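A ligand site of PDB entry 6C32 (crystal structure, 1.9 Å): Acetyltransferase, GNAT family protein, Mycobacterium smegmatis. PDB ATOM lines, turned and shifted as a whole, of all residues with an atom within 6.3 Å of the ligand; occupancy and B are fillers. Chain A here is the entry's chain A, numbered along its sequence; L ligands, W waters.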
ATOM      1  N   HIS A  42      -6.553  -5.420  -7.771  1.00  0.00           N
ATOM      2  CA  HIS A  42      -6.726  -6.477  -8.752  1.00  0.00           C
ATOM      3  C   HIS A  42      -5.413  -7.064  -9.252  1.00  0.00           C
ATOM      4  O   HIS A  42      -5.384  -8.206  -9.714  1.00  0.00           O
ATOM      5  CB  HIS A  42      -7.533  -5.957  -9.951  1.00  0.00           C
ATOM      6  CG  HIS A  42      -8.968  -5.645  -9.619  1.00  0.00           C
ATOM      7  ND1 HIS A  42      -9.437  -4.358  -9.464  1.00  0.00           N
ATOM      8  CD2 HIS A  42     -10.025  -6.463  -9.404  1.00  0.00           C
ATOM      9  CE1 HIS A  42     -10.727  -4.396  -9.174  1.00  0.00           C
ATOM     10  NE2 HIS A  42     -11.109  -5.664  -9.123  1.00  0.00           N
ATOM     11  N   LEU A  43      -4.318  -6.298  -9.163  1.00  0.00           N
ATOM     12  CA  LEU A  43      -3.034  -6.717  -9.717  1.00  0.00           C
ATOM     13  C   LEU A  43      -2.088  -7.284  -8.654  1.00  0.00           C
ATOM     14  O   LEU A  43      -1.441  -8.302  -8.908  1.00  0.00           O
ATOM     15  CB  LEU A  43      -2.343  -5.551 -10.424  1.00  0.00           C
ATOM     16  CG  LEU A  43      -3.070  -5.041 -11.667  1.00  0.00           C
ATOM     17  CD1 LEU A  43      -2.585  -3.639 -12.006  1.00  0.00           C
ATOM     18  CD2 LEU A  43      -2.871  -6.001 -12.839  1.00  0.00           C
ATOM     19  N   TRP A  46      -1.361 -11.057  -7.889  1.00  0.00           N
ATOM     20  CA  TRP A  46      -0.917 -11.895  -8.997  1.00  0.00           C
ATOM     21  C   TRP A  46       0.366 -11.381  -9.620  1.00  0.00           C
ATOM     22  O   TRP A  46       0.694 -11.763 -10.757  1.00  0.00           O
ATOM     23  CB  TRP A  46      -2.004 -11.978 -10.068  1.00  0.00           C
ATOM     24  CG  TRP A  46      -3.345 -12.239  -9.498  1.00  0.00           C
ATOM     25  CD1 TRP A  46      -4.399 -11.365  -9.407  1.00  0.00           C
ATOM     26  CD2 TRP A  46      -3.797 -13.467  -8.909  1.00  0.00           C
ATOM     27  NE1 TRP A  46      -5.481 -11.988  -8.817  1.00  0.00           N
ATOM     28  CE2 TRP A  46      -5.134 -13.268  -8.496  1.00  0.00           C
ATOM     29  CE3 TRP A  46      -3.193 -14.707  -8.700  1.00  0.00           C
ATOM     30  CZ2 TRP A  46      -5.876 -14.274  -7.881  1.00  0.00           C
ATOM     31  CZ3 TRP A  46      -3.935 -15.713  -8.084  1.00  0.00           C
ATOM     32  CH2 TRP A  46      -5.265 -15.487  -7.681  1.00  0.00           C
ATOM     33  N   GLU A  47       1.095 -10.521  -8.926  1.00  0.00           N
ATOM     34  CA  GLU A  47       2.264  -9.902  -9.524  1.00  0.00           C
ATOM     35  C   GLU A  47       3.482 -10.141  -8.649  1.00  0.00           C
ATOM     36  O   GLU A  47       3.383 -10.148  -7.422  1.00  0.00           O
ATOM     37  CB  GLU A  47       2.045  -8.400  -9.728  1.00  0.00           C
ATOM     38  CG  GLU A  47       1.050  -8.104 -10.829  1.00  0.00           C
ATOM     39  CD  GLU A  47       1.624  -7.171 -11.857  1.00  0.00           C
ATOM     40  OE1 GLU A  47       2.677  -6.573 -11.531  1.00  0.00           O
ATOM     41  OE2 GLU A  47       1.041  -7.053 -12.965  1.00  0.00           O
ATOM     42  N   ILE A 109       5.784 -15.868 -21.475  1.00  0.00           N
ATOM     43  CA  ILE A 109       4.822 -14.829 -21.855  1.00  0.00           C
ATOM     44  C   ILE A 109       3.987 -14.470 -20.632  1.00  0.00           C
ATOM     45  O   ILE A 109       3.618 -15.354 -19.844  1.00  0.00           O
ATOM     46  CB  ILE A 109       3.952 -15.286 -23.053  1.00  0.00           C
ATOM     47  CG1 ILE A 109       3.255 -14.088 -23.715  1.00  0.00           C
ATOM     48  CG2 ILE A 109       2.960 -16.391 -22.665  1.00  0.00           C
ATOM     49  CD1 ILE A 109       2.996 -14.306 -25.245  1.00  0.00           C
ATOM     50  N   GLY A 110       3.753 -13.168 -20.429  1.00  0.00           N
ATOM     51  CA  GLY A 110       2.928 -12.705 -19.327  1.00  0.00           C
ATOM     52  C   GLY A 110       2.073 -11.542 -19.785  1.00  0.00           C
ATOM     53  O   GLY A 110       2.347 -10.937 -20.819  1.00  0.00           O
ATOM     54  N   TYR A 111       1.030 -11.225 -19.011  1.00  0.00           N
ATOM     55  CA  TYR A 111       0.092 -10.200 -19.444  1.00  0.00           C
ATOM     56  C   TYR A 111      -0.734  -9.707 -18.264  1.00  0.00           C
ATOM     57  O   TYR A 111      -0.838 -10.364 -17.230  1.00  0.00           O
ATOM     58  CB  TYR A 111      -0.857 -10.730 -20.544  1.00  0.00           C
ATOM     59  CG  TYR A 111      -1.377 -12.106 -20.180  1.00  0.00           C
ATOM     60  CD1 TYR A 111      -2.448 -12.280 -19.306  1.00  0.00           C
ATOM     61  CD2 TYR A 111      -0.741 -13.246 -20.672  1.00  0.00           C
ATOM     62  CE1 TYR A 111      -2.896 -13.573 -18.949  1.00  0.00           C
ATOM     63  CE2 TYR A 111      -1.179 -14.514 -20.340  1.00  0.00           C
ATOM     64  CZ  TYR A 111      -2.250 -14.673 -19.475  1.00  0.00           C
ATOM     65  OH  TYR A 111      -2.637 -15.951 -19.151  1.00  0.00           O
ATOM     66  N   TRP A 112      -1.347  -8.541 -18.464  1.00  0.00           N
ATOM     67  CA  TRP A 112      -2.369  -8.051 -17.552  1.00  0.00           C
ATOM     68  C   TRP A 112      -3.245  -7.073 -18.329  1.00  0.00           C
ATOM     69  O   TRP A 112      -2.803  -6.450 -19.296  1.00  0.00           O
ATOM     70  CB  TRP A 112      -1.748  -7.383 -16.314  1.00  0.00           C
ATOM     71  CG  TRP A 112      -1.031  -6.090 -16.604  1.00  0.00           C
ATOM     72  CD1 TRP A 112       0.306  -5.933 -16.893  1.00  0.00           C
ATOM     73  CD2 TRP A 112      -1.593  -4.770 -16.617  1.00  0.00           C
ATOM     74  NE1 TRP A 112       0.595  -4.598 -17.087  1.00  0.00           N
ATOM     75  CE2 TRP A 112      -0.552  -3.855 -16.921  1.00  0.00           C
ATOM     76  CE3 TRP A 112      -2.886  -4.259 -16.392  1.00  0.00           C
ATOM     77  CZ2 TRP A 112      -0.762  -2.483 -17.014  1.00  0.00           C
ATOM     78  CZ3 TRP A 112      -3.101  -2.893 -16.497  1.00  0.00           C
ATOM     79  CH2 TRP A 112      -2.042  -2.020 -16.804  1.00  0.00           C
ATOM     80  N   VAL A 113      -4.498  -6.961 -17.895  1.00  0.00           N
ATOM     81  CA  VAL A 113      -5.485  -6.093 -18.532  1.00  0.00           C
ATOM     82  C   VAL A 113      -6.195  -5.300 -17.443  1.00  0.00           C
ATOM     83  O   VAL A 113      -6.534  -5.848 -16.387  1.00  0.00           O
ATOM     84  CB  VAL A 113      -6.513  -6.912 -19.364  1.00  0.00           C
ATOM     85  CG1 VAL A 113      -7.661  -6.018 -19.853  1.00  0.00           C
ATOM     86  CG2 VAL A 113      -5.838  -7.594 -20.576  1.00  0.00           C
ATOM     87  N   ALA A 114      -6.390  -4.001 -17.682  1.00  0.00           N
ATOM     88  CA  ALA A 114      -7.118  -3.148 -16.748  1.00  0.00           C
ATOM     89  C   ALA A 114      -8.455  -3.779 -16.364  1.00  0.00           C
ATOM     90  O   ALA A 114      -9.219  -4.201 -17.231  1.00  0.00           O
ATOM     91  CB  ALA A 114      -7.339  -1.770 -17.388  1.00  0.00           C
ATOM     92  N   SER A 115      -8.720  -3.833 -15.051  1.00  0.00           N
ATOM     93  CA  SER A 115      -9.862  -4.590 -14.551  1.00  0.00           C
ATOM     94  C   SER A 115     -11.179  -4.109 -15.148  1.00  0.00           C
ATOM     95  O   SER A 115     -12.090  -4.920 -15.383  1.00  0.00           O
ATOM     96  CB  SER A 115      -9.925  -4.522 -13.028  1.00  0.00           C
ATOM     97  OG  SER A 115     -10.117  -3.186 -12.604  1.00  0.00           O
ATOM     98  N   ARG A 117     -11.793  -3.346 -18.049  1.00  0.00           N
ATOM     99  CA  ARG A 117     -11.952  -3.876 -19.392  1.00  0.00           C
ATOM    100  C   ARG A 117     -11.919  -5.401 -19.458  1.00  0.00           C
ATOM    101  O   ARG A 117     -11.817  -5.961 -20.558  1.00  0.00           O
ATOM    102  CB  ARG A 117     -10.864  -3.312 -20.321  1.00  0.00           C
ATOM    103  CG  ARG A 117     -10.810  -1.811 -20.337  1.00  0.00           C
ATOM    104  CD  ARG A 117     -12.129  -1.233 -20.789  1.00  0.00           C
ATOM    105  NE  ARG A 117     -11.968   0.159 -21.167  1.00  0.00           N
ATOM    106  CZ  ARG A 117     -12.862   0.843 -21.879  1.00  0.00           C
ATOM    107  NH1 ARG A 117     -13.987   0.260 -22.260  1.00  0.00           N
ATOM    108  NH2 ARG A 117     -12.630   2.119 -22.181  1.00  0.00           N
ATOM    109  N   THR A 118     -11.995  -6.086 -18.309  1.00  0.00           N
ATOM    110  CA  THR A 118     -11.849  -7.529 -18.322  1.00  0.00           C
ATOM    111  C   THR A 118     -13.149  -8.195 -18.731  1.00  0.00           C
ATOM    112  O   THR A 118     -14.218  -7.575 -18.770  1.00  0.00           O
ATOM    113  CB  THR A 118     -11.405  -8.058 -16.951  1.00  0.00           C
ATOM    114  OG1 THR A 118     -12.248  -7.498 -15.937  1.00  0.00           O
ATOM    115  CG2 THR A 118      -9.944  -7.685 -16.672  1.00  0.00           C
ATOM    116  N   GLY A 119     -13.057  -9.490 -19.042  1.00  0.00           N
ATOM    117  CA  GLY A 119     -14.209 -10.260 -19.464  1.00  0.00           C
ATOM    118  C   GLY A 119     -14.679  -9.948 -20.861  1.00  0.00           C
ATOM    119  O   GLY A 119     -15.814 -10.296 -21.220  1.00  0.00           O
ATOM    120  N   GLY A 120     -13.853  -9.304 -21.673  1.00  0.00           N
ATOM    121  CA  GLY A 120     -14.223  -8.969 -23.039  1.00  0.00           C
ATOM    122  C   GLY A 120     -13.318  -9.601 -24.090  1.00  0.00           C
ATOM    123  O   GLY A 120     -13.383  -9.219 -25.265  1.00  0.00           O
ATOM    124  N   GLY A 121     -12.489 -10.566 -23.678  1.00  0.00           N
ATOM    125  CA  GLY A 121     -11.639 -11.296 -24.594  1.00  0.00           C
ATOM    126  C   GLY A 121     -10.317 -10.640 -24.942  1.00  0.00           C
ATOM    127  O   GLY A 121      -9.627 -11.118 -25.851  1.00  0.00           O
ATOM    128  N   ILE A 122      -9.933  -9.563 -24.231  1.00  0.00           N
ATOM    129  CA  ILE A 122      -8.727  -8.812 -24.583  1.00  0.00           C
ATOM    130  C   ILE A 122      -7.473  -9.638 -24.311  1.00  0.00           C
ATOM    131  O   ILE A 122      -6.599  -9.762 -25.172  1.00  0.00           O
ATOM    132  CB  ILE A 122      -8.681  -7.473 -23.831  1.00  0.00           C
ATOM    133  CG1 ILE A 122      -9.816  -6.551 -24.281  1.00  0.00           C
ATOM    134  CG2 ILE A 122      -7.304  -6.784 -23.998  1.00  0.00           C
ATOM    135  CD1 ILE A 122      -9.895  -5.252 -23.490  1.00  0.00           C
ATOM    136  N   ALA A 123      -7.335 -10.187 -23.094  1.00  0.00           N
ATOM    137  CA  ALA A 123      -6.124 -10.934 -22.770  1.00  0.00           C
ATOM    138  C   ALA A 123      -5.962 -12.142 -23.697  1.00  0.00           C
ATOM    139  O   ALA A 123      -4.841 -12.472 -24.120  1.00  0.00           O
ATOM    140  CB  ALA A 123      -6.139 -11.391 -21.308  1.00  0.00           C
ATOM    141  N   THR A 124      -7.068 -12.800 -24.011  1.00  0.00           N
ATOM    142  CA  THR A 124      -7.018 -13.958 -24.893  1.00  0.00           C
ATOM    143  C   THR A 124      -6.520 -13.573 -26.277  1.00  0.00           C
ATOM    144  O   THR A 124      -5.642 -14.245 -26.842  1.00  0.00           O
ATOM    145  CB  THR A 124      -8.396 -14.617 -24.973  1.00  0.00           C
ATOM    146  OG1 THR A 124      -8.744 -15.145 -23.685  1.00  0.00           O
ATOM    147  CG2 THR A 124      -8.353 -15.748 -25.961  1.00  0.00           C
ATOM    148  N   ALA A 125      -7.041 -12.460 -26.820  1.00  0.00           N
ATOM    149  CA  ALA A 125      -6.593 -11.974 -28.127  1.00  0.00           C
ATOM    150  C   ALA A 125      -5.148 -11.515 -28.077  1.00  0.00           C
ATOM    151  O   ALA A 125      -4.367 -11.809 -28.986  1.00  0.00           O
ATOM    152  CB  ALA A 125      -7.484 -10.827 -28.612  1.00  0.00           C
ATOM    153  N   ALA A 145       4.481 -20.271 -19.825  1.00  0.00           N
ATOM    154  CA  ALA A 145       3.957 -19.266 -18.903  1.00  0.00           C
ATOM    155  C   ALA A 145       3.885 -19.905 -17.523  1.00  0.00           C
ATOM    156  O   ALA A 145       3.770 -21.126 -17.412  1.00  0.00           O
ATOM    157  CB  ALA A 145       2.575 -18.742 -19.334  1.00  0.00           C
ATOM    158  N   THR A 146       3.992 -19.089 -16.487  1.00  0.00           N
ATOM    159  CA  THR A 146       3.785 -19.553 -15.120  1.00  0.00           C
ATOM    160  C   THR A 146       2.589 -18.805 -14.543  1.00  0.00           C
ATOM    161  O   THR A 146       2.404 -17.614 -14.788  1.00  0.00           O
ATOM    162  CB  THR A 146       5.026 -19.339 -14.244  1.00  0.00           C
ATOM    163  OG1 THR A 146       5.437 -17.967 -14.312  1.00  0.00           O
ATOM    164  CG2 THR A 146       6.162 -20.254 -14.706  1.00  0.00           C
ATOM    165  N   VAL A 147       1.783 -19.532 -13.761  1.00  0.00           N
ATOM    166  CA  VAL A 147       0.514 -18.992 -13.288  1.00  0.00           C
ATOM    167  C   VAL A 147       0.127 -19.714 -12.007  1.00  0.00           C
ATOM    168  O   VAL A 147       0.217 -20.948 -11.913  1.00  0.00           O
ATOM    169  CB  VAL A 147      -0.584 -19.109 -14.363  1.00  0.00           C
ATOM    170  CG1 VAL A 147      -0.768 -20.555 -14.802  1.00  0.00           C
ATOM    171  CG2 VAL A 147      -1.907 -18.486 -13.870  1.00  0.00           C
ATOM    172  N   ARG A 148      -0.275 -18.950 -10.988  1.00  0.00           N
ATOM    173  CA  ARG A 148      -0.688 -19.583  -9.736  1.00  0.00           C
ATOM    174  C   ARG A 148      -1.914 -20.461  -9.982  1.00  0.00           C
ATOM    175  O   ARG A 148      -2.817 -20.068 -10.747  1.00  0.00           O
ATOM    176  CB  ARG A 148      -0.993 -18.517  -8.680  1.00  0.00           C
ATOM    177  CG  ARG A 148       0.232 -17.710  -8.239  1.00  0.00           C
ATOM    178  CD  ARG A 148      -0.152 -16.706  -7.152  1.00  0.00           C
ATOM    179  NE  ARG A 148      -0.700 -17.333  -5.959  1.00  0.00           N
ATOM    180  CZ  ARG A 148      -1.277 -16.667  -4.960  1.00  0.00           C
ATOM    181  NH1 ARG A 148      -1.360 -15.338  -5.014  1.00  0.00           N
ATOM    182  NH2 ARG A 148      -1.759 -17.303  -3.908  1.00  0.00           N
ATOM    183  N   ASN A 151      -5.104 -18.684  -9.788  1.00  0.00           N
ATOM    184  CA  ASN A 151      -5.422 -17.646 -10.777  1.00  0.00           C
ATOM    185  C   ASN A 151      -6.300 -18.242 -11.879  1.00  0.00           C
ATOM    186  O   ASN A 151      -5.910 -18.403 -13.033  1.00  0.00           O
ATOM    187  CB  ASN A 151      -4.140 -17.042 -11.355  1.00  0.00           C
ATOM    188  CG  ASN A 151      -4.386 -15.728 -12.078  1.00  0.00           C
ATOM    189  OD1 ASN A 151      -5.526 -15.411 -12.420  1.00  0.00           O
ATOM    190  ND2 ASN A 151      -3.322 -14.946 -12.311  1.00  0.00           N
ATOM    191  N   THR A 152      -7.542 -18.580 -11.488  1.00  0.00           N
ATOM    192  CA  THR A 152      -8.473 -19.201 -12.417  1.00  0.00           C
ATOM    193  C   THR A 152      -8.726 -18.363 -13.668  1.00  0.00           C
ATOM    194  O   THR A 152      -8.801 -18.955 -14.762  1.00  0.00           O
ATOM    195  CB  THR A 152      -9.798 -19.490 -11.693  1.00  0.00           C
ATOM    196  OG1 THR A 152      -9.531 -20.058 -10.416  1.00  0.00           O
ATOM    197  CG2 THR A 152     -10.630 -20.474 -12.492  1.00  0.00           C
ATOM    198  N   PRO A 153      -8.885 -17.028 -13.599  1.00  0.00           N
ATOM    199  CA  PRO A 153      -9.054 -16.245 -14.845  1.00  0.00           C
ATOM    200  C   PRO A 153      -7.879 -16.373 -15.804  1.00  0.00           C
ATOM    201  O   PRO A 153      -8.092 -16.528 -17.011  1.00  0.00           O
ATOM    202  CB  PRO A 153      -9.201 -14.800 -14.354  1.00  0.00           C
ATOM    203  CG  PRO A 153      -9.567 -14.892 -12.927  1.00  0.00           C
ATOM    204  CD  PRO A 153      -8.943 -16.159 -12.403  1.00  0.00           C
ATOM    205  N   SER A 154      -6.647 -16.290 -15.306  1.00  0.00           N
ATOM    206  CA  SER A 154      -5.502 -16.400 -16.219  1.00  0.00           C
ATOM    207  C   SER A 154      -5.395 -17.793 -16.808  1.00  0.00           C
ATOM    208  O   SER A 154      -5.050 -17.957 -17.992  1.00  0.00           O
ATOM    209  CB  SER A 154      -4.201 -16.020 -15.500  1.00  0.00           C
ATOM    210  OG  SER A 154      -3.125 -16.057 -16.424  1.00  0.00           O
ATOM    211  N   ALA A 156      -7.859 -19.679 -17.527  1.00  0.00           N
ATOM    212  CA  ALA A 156      -8.857 -19.711 -18.603  1.00  0.00           C
ATOM    213  C   ALA A 156      -8.279 -19.114 -19.888  1.00  0.00           C
ATOM    214  O   ALA A 156      -8.422 -19.703 -20.964  1.00  0.00           O
ATOM    215  CB  ALA A 156     -10.117 -18.957 -18.173  1.00  0.00           C
ATOM    216  N   VAL A 157      -7.625 -17.950 -19.772  1.00  0.00           N
ATOM    217  CA  VAL A 157      -6.991 -17.316 -20.928  1.00  0.00           C
ATOM    218  C   VAL A 157      -6.019 -18.277 -21.606  1.00  0.00           C
ATOM    219  O   VAL A 157      -6.040 -18.456 -22.836  1.00  0.00           O
ATOM    220  CB  VAL A 157      -6.274 -16.020 -20.509  1.00  0.00           C
ATOM    221  CG1 VAL A 157      -5.418 -15.453 -21.660  1.00  0.00           C
ATOM    222  CG2 VAL A 157      -7.287 -14.981 -20.027  1.00  0.00           C
ATOM    223  N   LEU A 158      -5.148 -18.913 -20.816  1.00  0.00           N
ATOM    224  CA  LEU A 158      -4.156 -19.828 -21.373  1.00  0.00           C
ATOM    225  C   LEU A 158      -4.826 -21.029 -22.018  1.00  0.00           C
ATOM    226  O   LEU A 158      -4.387 -21.483 -23.084  1.00  0.00           O
ATOM    227  CB  LEU A 158      -3.183 -20.287 -20.268  1.00  0.00           C
ATOM    228  CG  LEU A 158      -2.309 -19.151 -19.698  1.00  0.00           C
ATOM    229  CD1 LEU A 158      -1.934 -19.402 -18.226  1.00  0.00           C
ATOM    230  CD2 LEU A 158      -1.066 -18.958 -20.575  1.00  0.00           C
ATOM    231  N   HIS A 160      -7.767 -21.048 -23.452  1.00  0.00           N
ATOM    232  CA  HIS A 160      -8.380 -20.594 -24.704  1.00  0.00           C
ATOM    233  C   HIS A 160      -7.444 -20.786 -25.887  1.00  0.00           C
ATOM    234  O   HIS A 160      -7.880 -21.101 -27.000  1.00  0.00           O
ATOM    235  CB  HIS A 160      -8.761 -19.119 -24.628  1.00  0.00           C
ATOM    236  CG  HIS A 160      -9.873 -18.825 -23.666  1.00  0.00           C
ATOM    237  ND1 HIS A 160     -10.154 -17.540 -23.237  1.00  0.00           N
ATOM    238  CD2 HIS A 160     -10.769 -19.631 -23.053  1.00  0.00           C
ATOM    239  CE1 HIS A 160     -11.175 -17.575 -22.400  1.00  0.00           C
ATOM    240  NE2 HIS A 160     -11.575 -18.837 -22.276  1.00  0.00           N
ATOM    241  N   ARG A 205     -14.426 -16.473 -30.525  1.00  0.00           N
ATOM    242  CA  ARG A 205     -13.895 -15.602 -29.481  1.00  0.00           C
ATOM    243  C   ARG A 205     -13.256 -14.337 -30.039  1.00  0.00           C
ATOM    244  O   ARG A 205     -12.894 -13.442 -29.263  1.00  0.00           O
ATOM    245  CB  ARG A 205     -12.878 -16.374 -28.617  1.00  0.00           C
ATOM    246  CG  ARG A 205     -13.542 -17.464 -27.758  1.00  0.00           C
ATOM    247  CD  ARG A 205     -12.603 -18.124 -26.735  1.00  0.00           C
ATOM    248  NE  ARG A 205     -13.373 -18.920 -25.778  1.00  0.00           N
ATOM    249  CZ  ARG A 205     -13.962 -18.422 -24.690  1.00  0.00           C
ATOM    250  NH1 ARG A 205     -13.880 -17.125 -24.392  1.00  0.00           N
ATOM    251  NH2 ARG A 205     -14.659 -19.224 -23.879  1.00  0.00           N
HETATM  252  N1  LIG L   1     -13.225 -18.445 -12.681  1.00  0.00           N
HETATM  253  C1  LIG L   1     -13.307 -18.966 -13.923  1.00  0.00           C
HETATM  254  N2  LIG L   1     -13.268 -18.188 -15.022  1.00  0.00           N
HETATM  255  C2  LIG L   1     -13.150 -16.834 -14.899  1.00  0.00           C
HETATM  256  C3  LIG L   1     -13.070 -16.256 -13.636  1.00  0.00           C
HETATM  257  C4  LIG L   1     -13.105 -17.128 -12.504  1.00  0.00           C
HETATM  258  N3  LIG L   1     -13.012 -16.557 -11.132  1.00  0.00           N
HETATM  259  N4  LIG L   1     -12.961 -14.950 -13.808  1.00  0.00           N
HETATM  260  C5  LIG L   1     -12.979 -14.711 -15.113  1.00  0.00           C
HETATM  261  N5  LIG L   1     -13.108 -15.852 -15.767  1.00  0.00           N
HETATM  262  C6  LIG L   1     -13.171 -16.035 -17.235  1.00  0.00           C
HETATM  263  C7  LIG L   1     -13.691 -15.072 -17.885  1.00  0.00           C
HETATM  264  O1  LIG L   1     -15.163 -15.125 -17.948  1.00  0.00           O
HETATM  265  C8  LIG L   1     -13.048 -15.302 -19.389  1.00  0.00           C
HETATM  266  O2  LIG L   1     -13.598 -16.517 -19.965  1.00  0.00           O
HETATM  267  P1  LIG L   1     -15.030 -16.604 -20.797  1.00  0.00           P
HETATM  268  O3  LIG L   1     -16.218 -16.363 -19.870  1.00  0.00           O
HETATM  269  O4  LIG L   1     -15.041 -18.005 -21.410  1.00  0.00           O
HETATM  270  O5  LIG L   1     -15.082 -15.553 -21.887  1.00  0.00           O
HETATM  271  C9  LIG L   1     -11.774 -15.551 -19.166  1.00  0.00           C
HETATM  272  O6  LIG L   1     -11.673 -15.994 -17.716  1.00  0.00           O
HETATM  273  C10 LIG L   1     -10.897 -14.263 -19.322  1.00  0.00           C
HETATM  274  O7  LIG L   1     -10.609 -14.257 -20.713  1.00  0.00           O
HETATM  275  P2  LIG L   1     -10.392 -12.778 -21.367  1.00  0.00           P
HETATM  276  O8  LIG L   1      -9.724 -12.929 -22.702  1.00  0.00           O
HETATM  277  O9  LIG L   1     -11.723 -12.061 -21.393  1.00  0.00           O
HETATM  278  O10 LIG L   1      -9.355 -12.112 -20.309  1.00  0.00           O
HETATM  279  P3  LIG L   1      -9.351 -10.619 -19.658  1.00  0.00           P
HETATM  280  O11 LIG L   1      -9.277  -9.565 -20.733  1.00  0.00           O
HETATM  281  O12 LIG L   1     -10.607 -10.528 -18.766  1.00  0.00           O
HETATM  282  O13 LIG L   1      -7.984 -10.563 -18.713  1.00  0.00           O
HETATM  283  C11 LIG L   1      -6.612 -11.303 -16.850  1.00  0.00           C
HETATM  284  C12 LIG L   1      -7.796 -11.660 -17.784  1.00  0.00           C
HETATM  285  C13 LIG L   1      -6.359 -12.479 -15.921  1.00  0.00           C
HETATM  286  C14 LIG L   1      -5.348 -11.042 -17.722  1.00  0.00           C
HETATM  287  C15 LIG L   1      -6.980 -10.045 -16.071  1.00  0.00           C
HETATM  288  O14 LIG L   1      -8.081 -10.328 -15.168  1.00  0.00           O
HETATM  289  C16 LIG L   1      -5.844  -9.516 -15.254  1.00  0.00           C
HETATM  290  O15 LIG L   1      -5.050  -8.724 -15.757  1.00  0.00           O
HETATM  291  N6  LIG L   1      -5.719  -9.959 -13.865  1.00  0.00           N
HETATM  292  C17 LIG L   1      -4.679  -9.509 -12.939  1.00  0.00           C
HETATM  293  C18 LIG L   1      -3.254  -9.767 -13.476  1.00  0.00           C
HETATM  294  C19 LIG L   1      -3.062 -11.258 -13.859  1.00  0.00           C
HETATM  295  O16 LIG L   1      -3.587 -12.178 -13.209  1.00  0.00           O
HETATM  296  N7  LIG L   1      -2.261 -11.550 -15.043  1.00  0.00           N
HETATM  297  C20 LIG L   1      -2.019 -12.988 -15.450  1.00  0.00           C
HETATM  298  C21 LIG L   1      -0.892 -13.485 -14.491  1.00  0.00           C
HETATM  299  S1  LIG L   1      -0.299 -15.091 -15.080  1.00  0.00           S
HETATM  300  C22 LIG L   1       0.409 -14.764 -16.734  1.00  0.00           C
HETATM  301  O17 LIG L   1       0.617 -13.647 -17.111  1.00  0.00           O
HETATM  302  C23 LIG L   1       0.742 -15.990 -17.637  1.00  0.00           C
HETATM  303  O   HOH W   1     -13.506 -13.638 -22.862  1.00  0.00           O
HETATM  304  O   HOH W   2     -15.962 -13.496 -15.769  1.00  0.00           O
HETATM  305  O   HOH W   3      -6.206 -12.666 -12.260  1.00  0.00           O
HETATM  306  O   HOH W   4       2.079 -15.436 -12.744  1.00  0.00           O
HETATM  307  O   HOH W   5     -10.381 -11.481 -14.752  1.00  0.00           O
HETATM  308  O   HOH W   6      -8.342  -8.288 -13.282  1.00  0.00           O
HETATM  309  O   HOH W   7     -11.222  -8.373 -21.824  1.00  0.00           O
HETATM  310  O   HOH W   8     -12.171 -11.638 -16.922  1.00  0.00           O
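A ring nitrogen (ND1) of His 42 sits at hydrogen-bond distance from the side-chain hydroxyl of Ser 115.
The side-chain hydroxyl (OG1) of Thr 118 lies within hydrogen-bond range of the backbone carbonyl oxygen (O) of Ser 115, at 2.6 Å.
OG1 of Thr 124 sits at hydrogen-bond distance from ND1 of His 160, 2.8 Å away.
A ring nitrogen (NE2) of His 160 sits close to the guanidinium group (NH2) of Arg 205, 3.5 Å away.
The side-chain hydroxyl of Ser 154 sits at hydrogen-bond distance from the side-chain hydroxyl of Tyr 111, 2.8 Å away.
The backbone NH of Ser 154 sits at hydrogen-bond distance from the side-chain amide oxygen of Asn 151, 3.2 Å away.
Water W8 bridges an oxygen (O12) of the ligand and the backbone NH of Gly 119.
Water W1 lies within hydrogen-bond range of O5 of the ligand (2.7 Å) and N of Gly 121 (3.3 Å).
Water W3 lies within hydrogen-bond range of an oxygen (O16) of the ligand and the side-chain amide oxygen (OD1) of Asn 151.
Water W4 bridges the backbone carbonyl oxygen of Thr 146 and a sulfur (S1) of the ligand.
N of Gly 120 lies within hydrogen-bond range of O9 of the ligand (3.5 Å).
S1 of the ligand sits close to OG of Ser 154, at 3.3 Å.
N of Val 113 sits at hydrogen-bond distance from O15 of the ligand (2.8 Å).
N of Gly 121 sits at hydrogen-bond distance from O9 of the ligand (2.8 Å).
An oxygen (O16) of the ligand is in hydrogen-bond range of the side-chain amide nitrogen (ND2) of Asn 151, at 2.9 Å.
An oxygen (O8) of the ligand sits at hydrogen-bond distance from the side-chain hydroxyl of Thr 124 (2.6 Å).
The backbone NH (N) of Gly 119 is in hydrogen-bond range of an oxygen (O12) of the ligand (2.7 Å).
An oxygen (O11) of the ligand is in hydrogen-bond range of the backbone NH (N) of Ala 123.
NH2 of Arg 205 is in salt-bridge range of O4 of the ligand.
The backbone NH of Tyr 111 sits at hydrogen-bond distance from an oxygen (O17) of the ligand (3.1 Å).
N7 of the ligand lies within hydrogen-bond range of O of Tyr 111, 2.9 Å away.
The backbone NH (N) of Thr 124 lies within hydrogen-bond range of an oxygen (O8) of the ligand (3.0 Å).
A sulfur (S1) of the ligand lies close to the backbone carbonyl oxygen (O) of Thr 146, 3.7 Å away.
His 42 touches the ligand.
Leu 43 touches the ligand.
CB of Trp 46 touches O16 of the ligand (3.5 Å).
Ile 109 touches the ligand.
CA of Gly 110 touches O17 of the ligand, at 3.3 Å.
Trp 112 touches the ligand (CA to O15, 3.3 Å).
Thr 118 touches the ligand (CB to O12, 3.2 Å).
N of Ile 122 touches O11 of the ligand (3.6 Å).
Ala 145 touches the ligand (CB to C23, 3.7 Å).
Val 147 touches the ligand.
Thr 152 touches the ligand (CG2 to N1, 3.3 Å).
Pro 153 touches the ligand.
CB of Ala 156 touches O6 of the ligand, 3.4 Å away.
Val 157 touches the ligand (CG2 to O7, 3.5 Å).
CE1 of His 160 touches O2 of the ligand (3.6 Å).
26 residues have an atom within 4 Å of the ligand: His 42, Leu 43, Trp 46, Ile 109, Gly 110, Tyr 111, Trp 112, Val 113, Thr 118, Gly 119, Gly 120, Gly 121, Ile 122, Ala 123, Thr 124, Ala 145, Thr 146, Val 147, Asn 151, Thr 152, Pro 153, Ser 154, Ala 156, Val 157, His 160 and Arg 205.
The nearest printed residue that does not touch the ligand is Leu 158 (4.4 Å).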
